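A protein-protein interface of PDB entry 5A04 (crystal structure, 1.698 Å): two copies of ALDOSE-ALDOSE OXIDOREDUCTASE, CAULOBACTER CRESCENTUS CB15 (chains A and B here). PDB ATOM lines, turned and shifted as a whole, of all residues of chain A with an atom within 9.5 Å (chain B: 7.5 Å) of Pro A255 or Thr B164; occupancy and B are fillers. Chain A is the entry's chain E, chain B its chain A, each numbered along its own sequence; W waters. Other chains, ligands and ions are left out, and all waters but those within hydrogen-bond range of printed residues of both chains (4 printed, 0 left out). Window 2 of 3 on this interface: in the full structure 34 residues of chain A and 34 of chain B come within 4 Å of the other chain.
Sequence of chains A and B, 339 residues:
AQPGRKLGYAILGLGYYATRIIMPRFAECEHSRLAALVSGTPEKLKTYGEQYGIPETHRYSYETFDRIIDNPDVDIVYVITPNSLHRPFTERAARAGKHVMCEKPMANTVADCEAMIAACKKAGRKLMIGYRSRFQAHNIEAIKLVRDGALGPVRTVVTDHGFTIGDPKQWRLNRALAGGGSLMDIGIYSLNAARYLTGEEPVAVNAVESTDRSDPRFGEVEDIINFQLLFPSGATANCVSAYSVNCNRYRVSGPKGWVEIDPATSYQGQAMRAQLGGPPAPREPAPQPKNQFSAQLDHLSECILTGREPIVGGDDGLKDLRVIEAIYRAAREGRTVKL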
ATOM      1  N   GLY A 149      25.738   4.937  17.331  1.00  0.00           N
ATOM      2  CA  GLY A 149      24.625   5.869  17.265  1.00  0.00           C
ATOM      3  C   GLY A 149      24.217   6.293  15.862  1.00  0.00           C
ATOM      4  O   GLY A 149      23.480   7.268  15.697  1.00  0.00           O
ATOM      5  N   ALA A 150      24.684   5.573  14.846  1.00  0.00           N
ATOM      6  CA  ALA A 150      24.421   5.972  13.468  1.00  0.00           C
ATOM      7  C   ALA A 150      22.933   5.931  13.133  1.00  0.00           C
ATOM      8  O   ALA A 150      22.473   6.647  12.239  1.00  0.00           O
ATOM      9  CB  ALA A 150      25.194   5.094  12.501  1.00  0.00           C
ATOM     10  N   LEU A 151      22.190   5.088  13.849  1.00  0.00           N
ATOM     11  CA  LEU A 151      20.763   4.899  13.565  1.00  0.00           C
ATOM     12  C   LEU A 151      19.868   5.611  14.566  1.00  0.00           C
ATOM     13  O   LEU A 151      18.651   5.647  14.398  1.00  0.00           O
ATOM     14  CB  LEU A 151      20.397   3.406  13.575  1.00  0.00           C
ATOM     15  CG  LEU A 151      21.284   2.392  12.855  1.00  0.00           C
ATOM     16  CD1 LEU A 151      20.566   1.030  12.809  1.00  0.00           C
ATOM     17  CD2 LEU A 151      21.650   2.860  11.468  1.00  0.00           C
ATOM     18  N   GLY A 152      20.462   6.142  15.627  1.00  0.00           N
ATOM     19  CA  GLY A 152      19.687   6.538  16.785  1.00  0.00           C
ATOM     20  C   GLY A 152      19.305   5.266  17.528  1.00  0.00           C
ATOM     21  O   GLY A 152      19.814   4.193  17.217  1.00  0.00           O
ATOM     22  N   PRO A 153      18.414   5.375  18.515  1.00  0.00           N
ATOM     23  CA  PRO A 153      17.969   4.189  19.264  1.00  0.00           C
ATOM     24  C   PRO A 153      17.351   3.139  18.344  1.00  0.00           C
ATOM     25  O   PRO A 153      16.610   3.510  17.431  1.00  0.00           O
ATOM     26  CB  PRO A 153      16.922   4.757  20.223  1.00  0.00           C
ATOM     27  CG  PRO A 153      17.316   6.198  20.379  1.00  0.00           C
ATOM     28  CD  PRO A 153      17.808   6.615  19.024  1.00  0.00           C
ATOM     29  N   VAL A 154      17.654   1.861  18.558  1.00  0.00           N
ATOM     30  CA  VAL A 154      17.055   0.822  17.722  1.00  0.00           C
ATOM     31  C   VAL A 154      15.546   0.791  17.965  1.00  0.00           C
ATOM     32  O   VAL A 154      15.093   0.720  19.113  1.00  0.00           O
ATOM     33  CB  VAL A 154      17.643  -0.568  18.006  1.00  0.00           C
ATOM     34  CG1 VAL A 154      16.889  -1.637  17.228  1.00  0.00           C
ATOM     35  CG2 VAL A 154      19.144  -0.600  17.689  1.00  0.00           C
ATOM     36  N   ARG A 155      14.770   0.845  16.885  1.00  0.00           N
ATOM     37  CA  ARG A 155      13.312   0.780  16.999  1.00  0.00           C
ATOM     38  C   ARG A 155      12.792  -0.544  16.455  1.00  0.00           C
ATOM     39  O   ARG A 155      11.929  -1.167  17.061  1.00  0.00           O
ATOM     40  CB  ARG A 155      12.643   1.942  16.251  1.00  0.00           C
ATOM     41  CG  ARG A 155      13.087   3.338  16.718  1.00  0.00           C
ATOM     42  CD  ARG A 155      12.631   3.611  18.149  1.00  0.00           C
ATOM     43  NE  ARG A 155      11.172   3.635  18.260  1.00  0.00           N
ATOM     44  CZ  ARG A 155      10.492   3.231  19.329  1.00  0.00           C
ATOM     45  NH1 ARG A 155      11.136   2.763  20.389  1.00  0.00           N
ATOM     46  NH2 ARG A 155       9.160   3.292  19.339  1.00  0.00           N
ATOM     47  N   THR A 156      13.294  -0.962  15.294  1.00  0.00           N
ATOM     48  CA  THR A 156      12.839  -2.225  14.712  1.00  0.00           C
ATOM     49  C   THR A 156      13.995  -3.072  14.222  1.00  0.00           C
ATOM     50  O   THR A 156      14.987  -2.553  13.707  1.00  0.00           O
ATOM     51  CB  THR A 156      11.876  -2.013  13.514  1.00  0.00           C
ATOM     52  OG1 THR A 156      12.566  -1.322  12.460  1.00  0.00           O
ATOM     53  CG2 THR A 156      10.626  -1.218  13.922  1.00  0.00           C
ATOM     54  N   VAL A 252      18.088  -3.528  10.554  1.00  0.00           N
ATOM     55  CA  VAL A 252      17.861  -2.862  11.835  1.00  0.00           C
ATOM     56  C   VAL A 252      17.697  -1.366  11.566  1.00  0.00           C
ATOM     57  O   VAL A 252      18.447  -0.778  10.771  1.00  0.00           O
ATOM     58  CB  VAL A 252      19.009  -3.162  12.850  1.00  0.00           C
ATOM     59  CG1 VAL A 252      20.376  -2.860  12.249  1.00  0.00           C
ATOM     60  CG2 VAL A 252      18.807  -2.424  14.165  1.00  0.00           C
ATOM     61  N   SER A 253      16.669  -0.768  12.173  1.00  0.00           N
ATOM     62  CA  SER A 253      16.279   0.612  11.859  1.00  0.00           C
ATOM     63  C   SER A 253      16.065   1.449  13.105  1.00  0.00           C
ATOM     64  O   SER A 253      15.545   0.958  14.119  1.00  0.00           O
ATOM     65  CB  SER A 253      14.984   0.641  11.021  1.00  0.00           C
ATOM     66  OG  SER A 253      15.053  -0.230   9.900  1.00  0.00           O
ATOM     67  N   GLY A 254      16.451   2.721  13.019  1.00  0.00           N
ATOM     68  CA  GLY A 254      16.213   3.693  14.077  1.00  0.00           C
ATOM     69  C   GLY A 254      15.776   5.007  13.425  1.00  0.00           C
ATOM     70  O   GLY A 254      15.656   5.082  12.203  1.00  0.00           O
ATOM     71  N   PRO A 255      15.552   6.053  14.234  1.00  0.00           N
ATOM     72  CA  PRO A 255      15.021   7.311  13.697  1.00  0.00           C
ATOM     73  C   PRO A 255      15.960   7.989  12.692  1.00  0.00           C
ATOM     74  O   PRO A 255      15.498   8.802  11.884  1.00  0.00           O
ATOM     75  CB  PRO A 255      14.857   8.192  14.948  1.00  0.00           C
ATOM     76  CG  PRO A 255      14.827   7.253  16.092  1.00  0.00           C
ATOM     77  CD  PRO A 255      15.665   6.070  15.702  1.00  0.00           C
ATOM     78  N   LYS A 256      17.254   7.664  12.748  1.00  0.00           N
ATOM     79  CA  LYS A 256      18.240   8.339  11.905  1.00  0.00           C
ATOM     80  C   LYS A 256      18.552   7.581  10.621  1.00  0.00           C
ATOM     81  O   LYS A 256      19.186   8.122   9.709  1.00  0.00           O
ATOM     82  CB  LYS A 256      19.534   8.568  12.686  1.00  0.00           C
ATOM     83  CG  LYS A 256      19.405   9.568  13.820  1.00  0.00           C
ATOM     84  CD  LYS A 256      20.757   9.748  14.492  1.00  0.00           C
ATOM     85  CE  LYS A 256      20.656  10.686  15.682  1.00  0.00           C
ATOM     86  NZ  LYS A 256      21.983  10.829  16.355  1.00  0.00           N
ATOM     87  N   GLY A 257      18.114   6.328  10.533  1.00  0.00           N
ATOM     88  CA  GLY A 257      18.390   5.556   9.340  1.00  0.00           C
ATOM     89  C   GLY A 257      18.412   4.073   9.621  1.00  0.00           C
ATOM     90  O   GLY A 257      18.036   3.644  10.713  1.00  0.00           O
ATOM     91  N   TRP A 258      18.828   3.289   8.634  1.00  0.00           N
ATOM     92  CA  TRP A 258      18.832   1.852   8.822  1.00  0.00           C
ATOM     93  C   TRP A 258      19.982   1.171   8.113  1.00  0.00           C
ATOM     94  O   TRP A 258      20.663   1.768   7.261  1.00  0.00           O
ATOM     95  CB  TRP A 258      17.496   1.245   8.373  1.00  0.00           C
ATOM     96  CG  TRP A 258      16.961   1.555   6.973  1.00  0.00           C
ATOM     97  CD1 TRP A 258      15.923   2.396   6.668  1.00  0.00           C
ATOM     98  CD2 TRP A 258      17.353   0.941   5.732  1.00  0.00           C
ATOM     99  NE1 TRP A 258      15.664   2.358   5.312  1.00  0.00           N
ATOM    100  CE2 TRP A 258      16.531   1.482   4.717  1.00  0.00           C
ATOM    101  CE3 TRP A 258      18.339   0.009   5.375  1.00  0.00           C
ATOM    102  CZ2 TRP A 258      16.668   1.126   3.372  1.00  0.00           C
ATOM    103  CZ3 TRP A 258      18.474  -0.342   4.041  1.00  0.00           C
ATOM    104  CH2 TRP A 258      17.628   0.206   3.058  1.00  0.00           C
ATOM    105  N   GLN A 275      20.843   3.056   4.779  1.00  0.00           N
ATOM    106  CA  GLN A 275      20.161   4.303   4.477  1.00  0.00           C
ATOM    107  C   GLN A 275      20.497   5.259   5.608  1.00  0.00           C
ATOM    108  O   GLN A 275      19.949   5.157   6.709  1.00  0.00           O
ATOM    109  CB  GLN A 275      18.650   4.078   4.333  1.00  0.00           C
ATOM    110  CG  GLN A 275      17.873   5.252   3.770  1.00  0.00           C
ATOM    111  CD  GLN A 275      17.549   6.263   4.830  1.00  0.00           C
ATOM    112  OE1 GLN A 275      16.726   6.011   5.709  1.00  0.00           O
ATOM    113  NE2 GLN A 275      18.209   7.415   4.773  1.00  0.00           N
ATOM    114  N   LEU A 276      21.454   6.154   5.350  1.00  0.00           N
ATOM    115  CA  LEU A 276      21.955   7.057   6.376  1.00  0.00           C
ATOM    116  C   LEU A 276      22.044   8.480   5.844  1.00  0.00           C
ATOM    117  O   LEU A 276      23.054   8.867   5.253  1.00  0.00           O
ATOM    118  CB  LEU A 276      23.333   6.595   6.865  1.00  0.00           C
ATOM    119  CG  LEU A 276      23.441   5.164   7.390  1.00  0.00           C
ATOM    120  CD1 LEU A 276      24.894   4.709   7.437  1.00  0.00           C
ATOM    121  CD2 LEU A 276      22.800   5.065   8.769  1.00  0.00           C
ATOM    122  N   GLY A 277      20.986   9.257   6.041  1.00  0.00           N
ATOM    123  CA  GLY A 277      20.959  10.624   5.546  1.00  0.00           C
ATOM    124  C   GLY A 277      20.441  10.752   4.124  1.00  0.00           C
ATOM    125  O   GLY A 277      19.646  11.642   3.827  1.00  0.00           O
ATOM    126  N   GLY B 162       6.465   2.630   7.355  1.00  0.00           N
ATOM    127  CA  GLY B 162       6.613   3.623   8.395  1.00  0.00           C
ATOM    128  C   GLY B 162       7.316   4.846   7.859  1.00  0.00           C
ATOM    129  O   GLY B 162       7.980   4.787   6.813  1.00  0.00           O
ATOM    130  N   PHE B 163       7.150   5.965   8.542  1.00  0.00           N
ATOM    131  CA  PHE B 163       7.980   7.131   8.262  1.00  0.00           C
ATOM    132  C   PHE B 163       8.190   7.886   9.561  1.00  0.00           C
ATOM    133  O   PHE B 163       7.459   7.700  10.527  1.00  0.00           O
ATOM    134  CB  PHE B 163       7.376   8.032   7.173  1.00  0.00           C
ATOM    135  CG  PHE B 163       6.115   8.759   7.580  1.00  0.00           C
ATOM    136  CD1 PHE B 163       4.877   8.138   7.492  1.00  0.00           C
ATOM    137  CD2 PHE B 163       6.171  10.085   7.998  1.00  0.00           C
ATOM    138  CE1 PHE B 163       3.719   8.822   7.843  1.00  0.00           C
ATOM    139  CE2 PHE B 163       5.016  10.774   8.357  1.00  0.00           C
ATOM    140  CZ  PHE B 163       3.794  10.139   8.275  1.00  0.00           C
ATOM    141  N   THR B 164       9.223   8.712   9.594  1.00  0.00           N
ATOM    142  CA  THR B 164       9.530   9.467  10.792  1.00  0.00           C
ATOM    143  C   THR B 164       8.677  10.714  10.814  1.00  0.00           C
ATOM    144  O   THR B 164       9.022  11.717  10.199  1.00  0.00           O
ATOM    145  CB  THR B 164      11.023   9.835  10.840  1.00  0.00           C
ATOM    146  OG1 THR B 164      11.413  10.358   9.564  1.00  0.00           O
ATOM    147  CG2 THR B 164      11.845   8.601  11.114  1.00  0.00           C
ATOM    148  N   ILE B 165       7.546  10.648  11.510  1.00  0.00           N
ATOM    149  CA  ILE B 165       6.602  11.756  11.495  1.00  0.00           C
ATOM    150  C   ILE B 165       7.175  12.947  12.281  1.00  0.00           C
ATOM    151  O   ILE B 165       7.980  12.767  13.192  1.00  0.00           O
ATOM    152  CB  ILE B 165       5.227  11.306  12.056  1.00  0.00           C
ATOM    153  CG1 ILE B 165       4.127  12.304  11.661  1.00  0.00           C
ATOM    154  CG2 ILE B 165       5.302  11.039  13.558  1.00  0.00           C
ATOM    155  CD1 ILE B 165       2.713  11.756  11.882  1.00  0.00           C
ATOM    156  N   GLY B 166       6.781  14.161  11.903  1.00  0.00           N
ATOM    157  CA  GLY B 166       7.404  15.353  12.462  1.00  0.00           C
ATOM    158  C   GLY B 166       6.587  16.151  13.466  1.00  0.00           C
ATOM    159  O   GLY B 166       6.588  15.856  14.665  1.00  0.00           O
ATOM    160  N   ASP B 167       5.890  17.170  12.966  1.00  0.00           N
ATOM    161  CA  ASP B 167       5.189  18.147  13.806  1.00  0.00           C
ATOM    162  C   ASP B 167       4.162  17.506  14.742  1.00  0.00           C
ATOM    163  O   ASP B 167       3.163  16.974  14.278  1.00  0.00           O
ATOM    164  CB  ASP B 167       4.496  19.175  12.901  1.00  0.00           C
ATOM    165  CG  ASP B 167       3.870  20.333  13.671  1.00  0.00           C
ATOM    166  OD1 ASP B 167       3.814  20.298  14.917  1.00  0.00           O
ATOM    167  OD2 ASP B 167       3.429  21.293  13.007  1.00  0.00           O
ATOM    168  N   GLN B 170       0.154  18.157  14.309  1.00  0.00           N
ATOM    169  CA  GLN B 170      -0.601  17.821  13.106  1.00  0.00           C
ATOM    170  C   GLN B 170      -1.733  16.835  13.403  1.00  0.00           C
ATOM    171  O   GLN B 170      -1.687  16.113  14.401  1.00  0.00           O
ATOM    172  CB  GLN B 170       0.327  17.241  12.050  1.00  0.00           C
ATOM    173  CG  GLN B 170       0.832  15.847  12.380  1.00  0.00           C
ATOM    174  CD  GLN B 170       1.863  15.380  11.382  1.00  0.00           C
ATOM    175  OE1 GLN B 170       1.521  14.882  10.308  1.00  0.00           O
ATOM    176  NE2 GLN B 170       3.141  15.551  11.725  1.00  0.00           N
ATOM    177  N   ARG B 217       5.399  13.750  20.323  1.00  0.00           N
ATOM    178  CA  ARG B 217       4.552  13.343  19.204  1.00  0.00           C
ATOM    179  C   ARG B 217       3.460  12.357  19.623  1.00  0.00           C
ATOM    180  O   ARG B 217       2.438  12.230  18.948  1.00  0.00           O
ATOM    181  CB  ARG B 217       5.394  12.691  18.107  1.00  0.00           C
ATOM    182  CG  ARG B 217       6.333  13.626  17.383  1.00  0.00           C
ATOM    183  CD  ARG B 217       7.222  12.831  16.419  1.00  0.00           C
ATOM    184  NE  ARG B 217       8.188  11.998  17.131  1.00  0.00           N
ATOM    185  CZ  ARG B 217       8.980  11.089  16.560  1.00  0.00           C
ATOM    186  NH1 ARG B 217       8.938  10.877  15.248  1.00  0.00           N
ATOM    187  NH2 ARG B 217       9.828  10.385  17.311  1.00  0.00           N
ATOM    188  N   PHE B 218       3.695  11.635  20.716  1.00  0.00           N
ATOM    189  CA  PHE B 218       2.931  10.411  20.953  1.00  0.00           C
ATOM    190  C   PHE B 218       2.170  10.409  22.284  1.00  0.00           C
ATOM    191  O   PHE B 218       2.134   9.401  22.981  1.00  0.00           O
ATOM    192  CB  PHE B 218       3.869   9.199  20.878  1.00  0.00           C
ATOM    193  CG  PHE B 218       4.600   9.066  19.555  1.00  0.00           C
ATOM    194  CD1 PHE B 218       3.907   9.063  18.356  1.00  0.00           C
ATOM    195  CD2 PHE B 218       5.985   8.947  19.524  1.00  0.00           C
ATOM    196  CE1 PHE B 218       4.581   8.943  17.136  1.00  0.00           C
ATOM    197  CE2 PHE B 218       6.668   8.836  18.320  1.00  0.00           C
ATOM    198  CZ  PHE B 218       5.970   8.827  17.122  1.00  0.00           C
ATOM    199  N   ASP B 223       3.003   4.819  18.192  1.00  0.00           N
ATOM    200  CA  ASP B 223       4.149   4.939  17.301  1.00  0.00           C
ATOM    201  C   ASP B 223       4.328   3.625  16.548  1.00  0.00           C
ATOM    202  O   ASP B 223       3.964   3.533  15.377  1.00  0.00           O
ATOM    203  CB  ASP B 223       5.400   5.304  18.104  1.00  0.00           C
ATOM    204  CG  ASP B 223       6.679   5.212  17.283  1.00  0.00           C
ATOM    205  OD1 ASP B 223       6.601   5.142  16.040  1.00  0.00           O
ATOM    206  OD2 ASP B 223       7.760   5.231  17.898  1.00  0.00           O
ATOM    207  N   ALA B 242       5.011   1.914  11.742  1.00  0.00           N
ATOM    208  CA  ALA B 242       5.834   2.764  12.602  1.00  0.00           C
ATOM    209  C   ALA B 242       5.763   4.247  12.235  1.00  0.00           C
ATOM    210  O   ALA B 242       5.593   4.609  11.073  1.00  0.00           O
ATOM    211  CB  ALA B 242       7.297   2.287  12.559  1.00  0.00           C
ATOM    212  N   TYR B 243       5.917   5.091  13.248  1.00  0.00           N
ATOM    213  CA  TYR B 243       6.004   6.532  13.063  1.00  0.00           C
ATOM    214  C   TYR B 243       7.395   7.055  13.456  1.00  0.00           C
ATOM    215  O   TYR B 243       7.606   8.266  13.526  1.00  0.00           O
ATOM    216  CB  TYR B 243       4.930   7.241  13.897  1.00  0.00           C
ATOM    217  CG  TYR B 243       3.643   7.624  13.174  1.00  0.00           C
ATOM    218  CD1 TYR B 243       3.572   7.692  11.789  1.00  0.00           C
ATOM    219  CD2 TYR B 243       2.500   7.952  13.902  1.00  0.00           C
ATOM    220  CE1 TYR B 243       2.396   8.077  11.149  1.00  0.00           C
ATOM    221  CE2 TYR B 243       1.328   8.338  13.276  1.00  0.00           C
ATOM    222  CZ  TYR B 243       1.272   8.399  11.904  1.00  0.00           C
ATOM    223  OH  TYR B 243       0.096   8.794  11.306  1.00  0.00           O
ATOM    224  N   SER B 244       8.327   6.153  13.752  1.00  0.00           N
ATOM    225  CA  SER B 244       9.662   6.566  14.203  1.00  0.00           C
ATOM    226  C   SER B 244      10.801   5.964  13.371  1.00  0.00           C
ATOM    227  O   SER B 244      11.971   6.163  13.692  1.00  0.00           O
ATOM    228  CB  SER B 244       9.865   6.224  15.690  1.00  0.00           C
ATOM    229  OG  SER B 244       9.718   4.830  15.947  1.00  0.00           O
ATOM    230  N   VAL B 245      10.469   5.233  12.311  1.00  0.00           N
ATOM    231  CA  VAL B 245      11.480   4.785  11.342  1.00  0.00           C
ATOM    232  C   VAL B 245      10.934   4.920   9.933  1.00  0.00           C
ATOM    233  O   VAL B 245       9.726   4.997   9.739  1.00  0.00           O
ATOM    234  CB  VAL B 245      11.921   3.313  11.553  1.00  0.00           C
ATOM    235  CG1 VAL B 245      12.548   3.112  12.917  1.00  0.00           C
ATOM    236  CG2 VAL B 245      10.752   2.354  11.347  1.00  0.00           C
ATOM    237  N   ASN B 246      11.824   4.934   8.946  1.00  0.00           N
ATOM    238  CA  ASN B 246      11.393   4.931   7.552  1.00  0.00           C
ATOM    239  C   ASN B 246      11.536   3.555   6.909  1.00  0.00           C
ATOM    240  O   ASN B 246      12.617   2.965   6.898  1.00  0.00           O
ATOM    241  CB  ASN B 246      12.188   5.958   6.743  1.00  0.00           C
ATOM    242  CG  ASN B 246      11.938   7.373   7.211  1.00  0.00           C
ATOM    243  OD1 ASN B 246      10.820   7.885   7.101  1.00  0.00           O
ATOM    244  ND2 ASN B 246      12.975   8.013   7.740  1.00  0.00           N
ATOM    245  N   CYS B 247      10.434   3.048   6.370  1.00  0.00           N
ATOM    246  CA  CYS B 247      10.448   1.790   5.657  1.00  0.00           C
ATOM    247  C   CYS B 247       9.252   1.718   4.743  1.00  0.00           C
ATOM    248  O   CYS B 247       8.197   2.275   5.035  1.00  0.00           O
ATOM    249  CB  CYS B 247      10.433   0.600   6.617  1.00  0.00           C
ATOM    250  SG  CYS B 247       9.191   0.719   7.954  1.00  0.00           S
HETATM  251  O   HOH W   1      14.629   4.745   9.582  1.00  0.00           O
HETATM  252  O   HOH W   2      15.635   6.922   7.894  1.00  0.00           O
HETATM  253  O   HOH W   3      13.339   0.453   7.715  1.00  0.00           O
HETATM  254  O   HOH W   4       7.939   6.170  20.408  1.00  0.00           O
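The side-chain carboxylate (OD2) of Asp B223 is in salt-bridge range of the guanidinium group (NH2) of Arg A155, 2.8 Å away.
NE of Arg A155 is in hydrogen-bond range of OG of Ser B244.
The indole nitrogen (NE1) of Trp A258 sits close to the backbone carbonyl oxygen (O) of Asn B246 (3.5 Å).
The backbone carbonyl oxygen of Val B245 is in hydrogen-bond range of the backbone NH of Phe B163 (3.0 Å).
N of Thr B164 lies within hydrogen-bond range of OD1 of Asn B246.
The side-chain carboxylate of Asp B223 lies within hydrogen-bond range of the backbone NH of Tyr B243 (2.9 Å).
OG of Ser B244 sits at hydrogen-bond distance from OD2 of Asp B223, at 2.8 Å.
The backbone NH (N) of Arg A155 lies within hydrogen-bond range of the backbone carbonyl oxygen (O) of Ser A253 (2.9 Å).
The backbone NH (N) of Gln A275 is in hydrogen-bond range of the backbone carbonyl oxygen (O) of Trp A258, 2.8 Å away.
Val B245 touches Arg A155.
Ser A253 touches Val B245 (O to CG1, 3.9 Å).
Ser B244 touches Gly A254 (O to C, 3.99 Å).
Gly A254 touches Val B245.
Thr B164 touches Pro A255.
O of Ser B244 touches CA of Pro A255, at 3.3 Å.
Of the printed residues of chain B, Pro A255 touches Thr B164 and Ser B244.
Printed residues of chain A within 4 Å of Asn B246: Trp A258 (3.4 Å).
Printed residues of chain A within 4 Å of Val B245: Arg A155 (3.5 Å), Ser A253 (3.9 Å) and Gly A254 (3.7 Å).
Printed residues of chain B within 4 Å of Gly A254: Ser B244 (3.99 Å) and Val B245 (3.7 Å).
Of the printed residues of chain B, Trp A258 touches Asn B246 (3.4 Å).
Printed residues of chain B within 4 Å of Arg A155: Asp B223 (2.8 Å), Ser B244 (3.0 Å) and Val B245 (3.5 Å).
The nearest residue of chain A that does not touch Thr B164 is Gly A254 (5.3 Å).
The nearest printed residue of chain A that does not touch Ser B244 is Lys A256 (5.6 Å).
Of the 16 printed residues of chain B, 5 touch a printed residue of chain A.
Hydrophobic or aromatic side chains of chain B that line the printed part of chain A: Val B245.
Of the 18 printed residues of chain A, 5 touch a printed residue of chain B.
Among the printed residues, 9 pairs touch across the chains.
Among the printed residues, Asp or Glu carboxylates within 4 Å of a Lys or Arg side-chain nitrogen of the other chain: Arg A155 with Asp B223.
No position is printed for both chains.
Of the 9 pairs that touch across the chains among the printed residues, none has its exchanged pair printed and touching as well.
Water W2 lies within hydrogen-bond range of OE1 of Gln A275 (2.6 Å) and ND2 of Asn B246 (2.9 Å).
Water W4 lies within hydrogen-bond range of the side-chain carboxylate of Asp B223 (2.7 Å) and the guanidinium group of Arg A155 (3.3 Å).
Water W3 bridges the backbone carbonyl oxygen (O) of Asn B246 (2.7 Å) and the side-chain hydroxyl (OG) of Ser A253 (2.9 Å).
Water W1 lies within hydrogen-bond range of O of Gly A254 (2.8 Å) and N of Asn B246 (2.9 Å).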
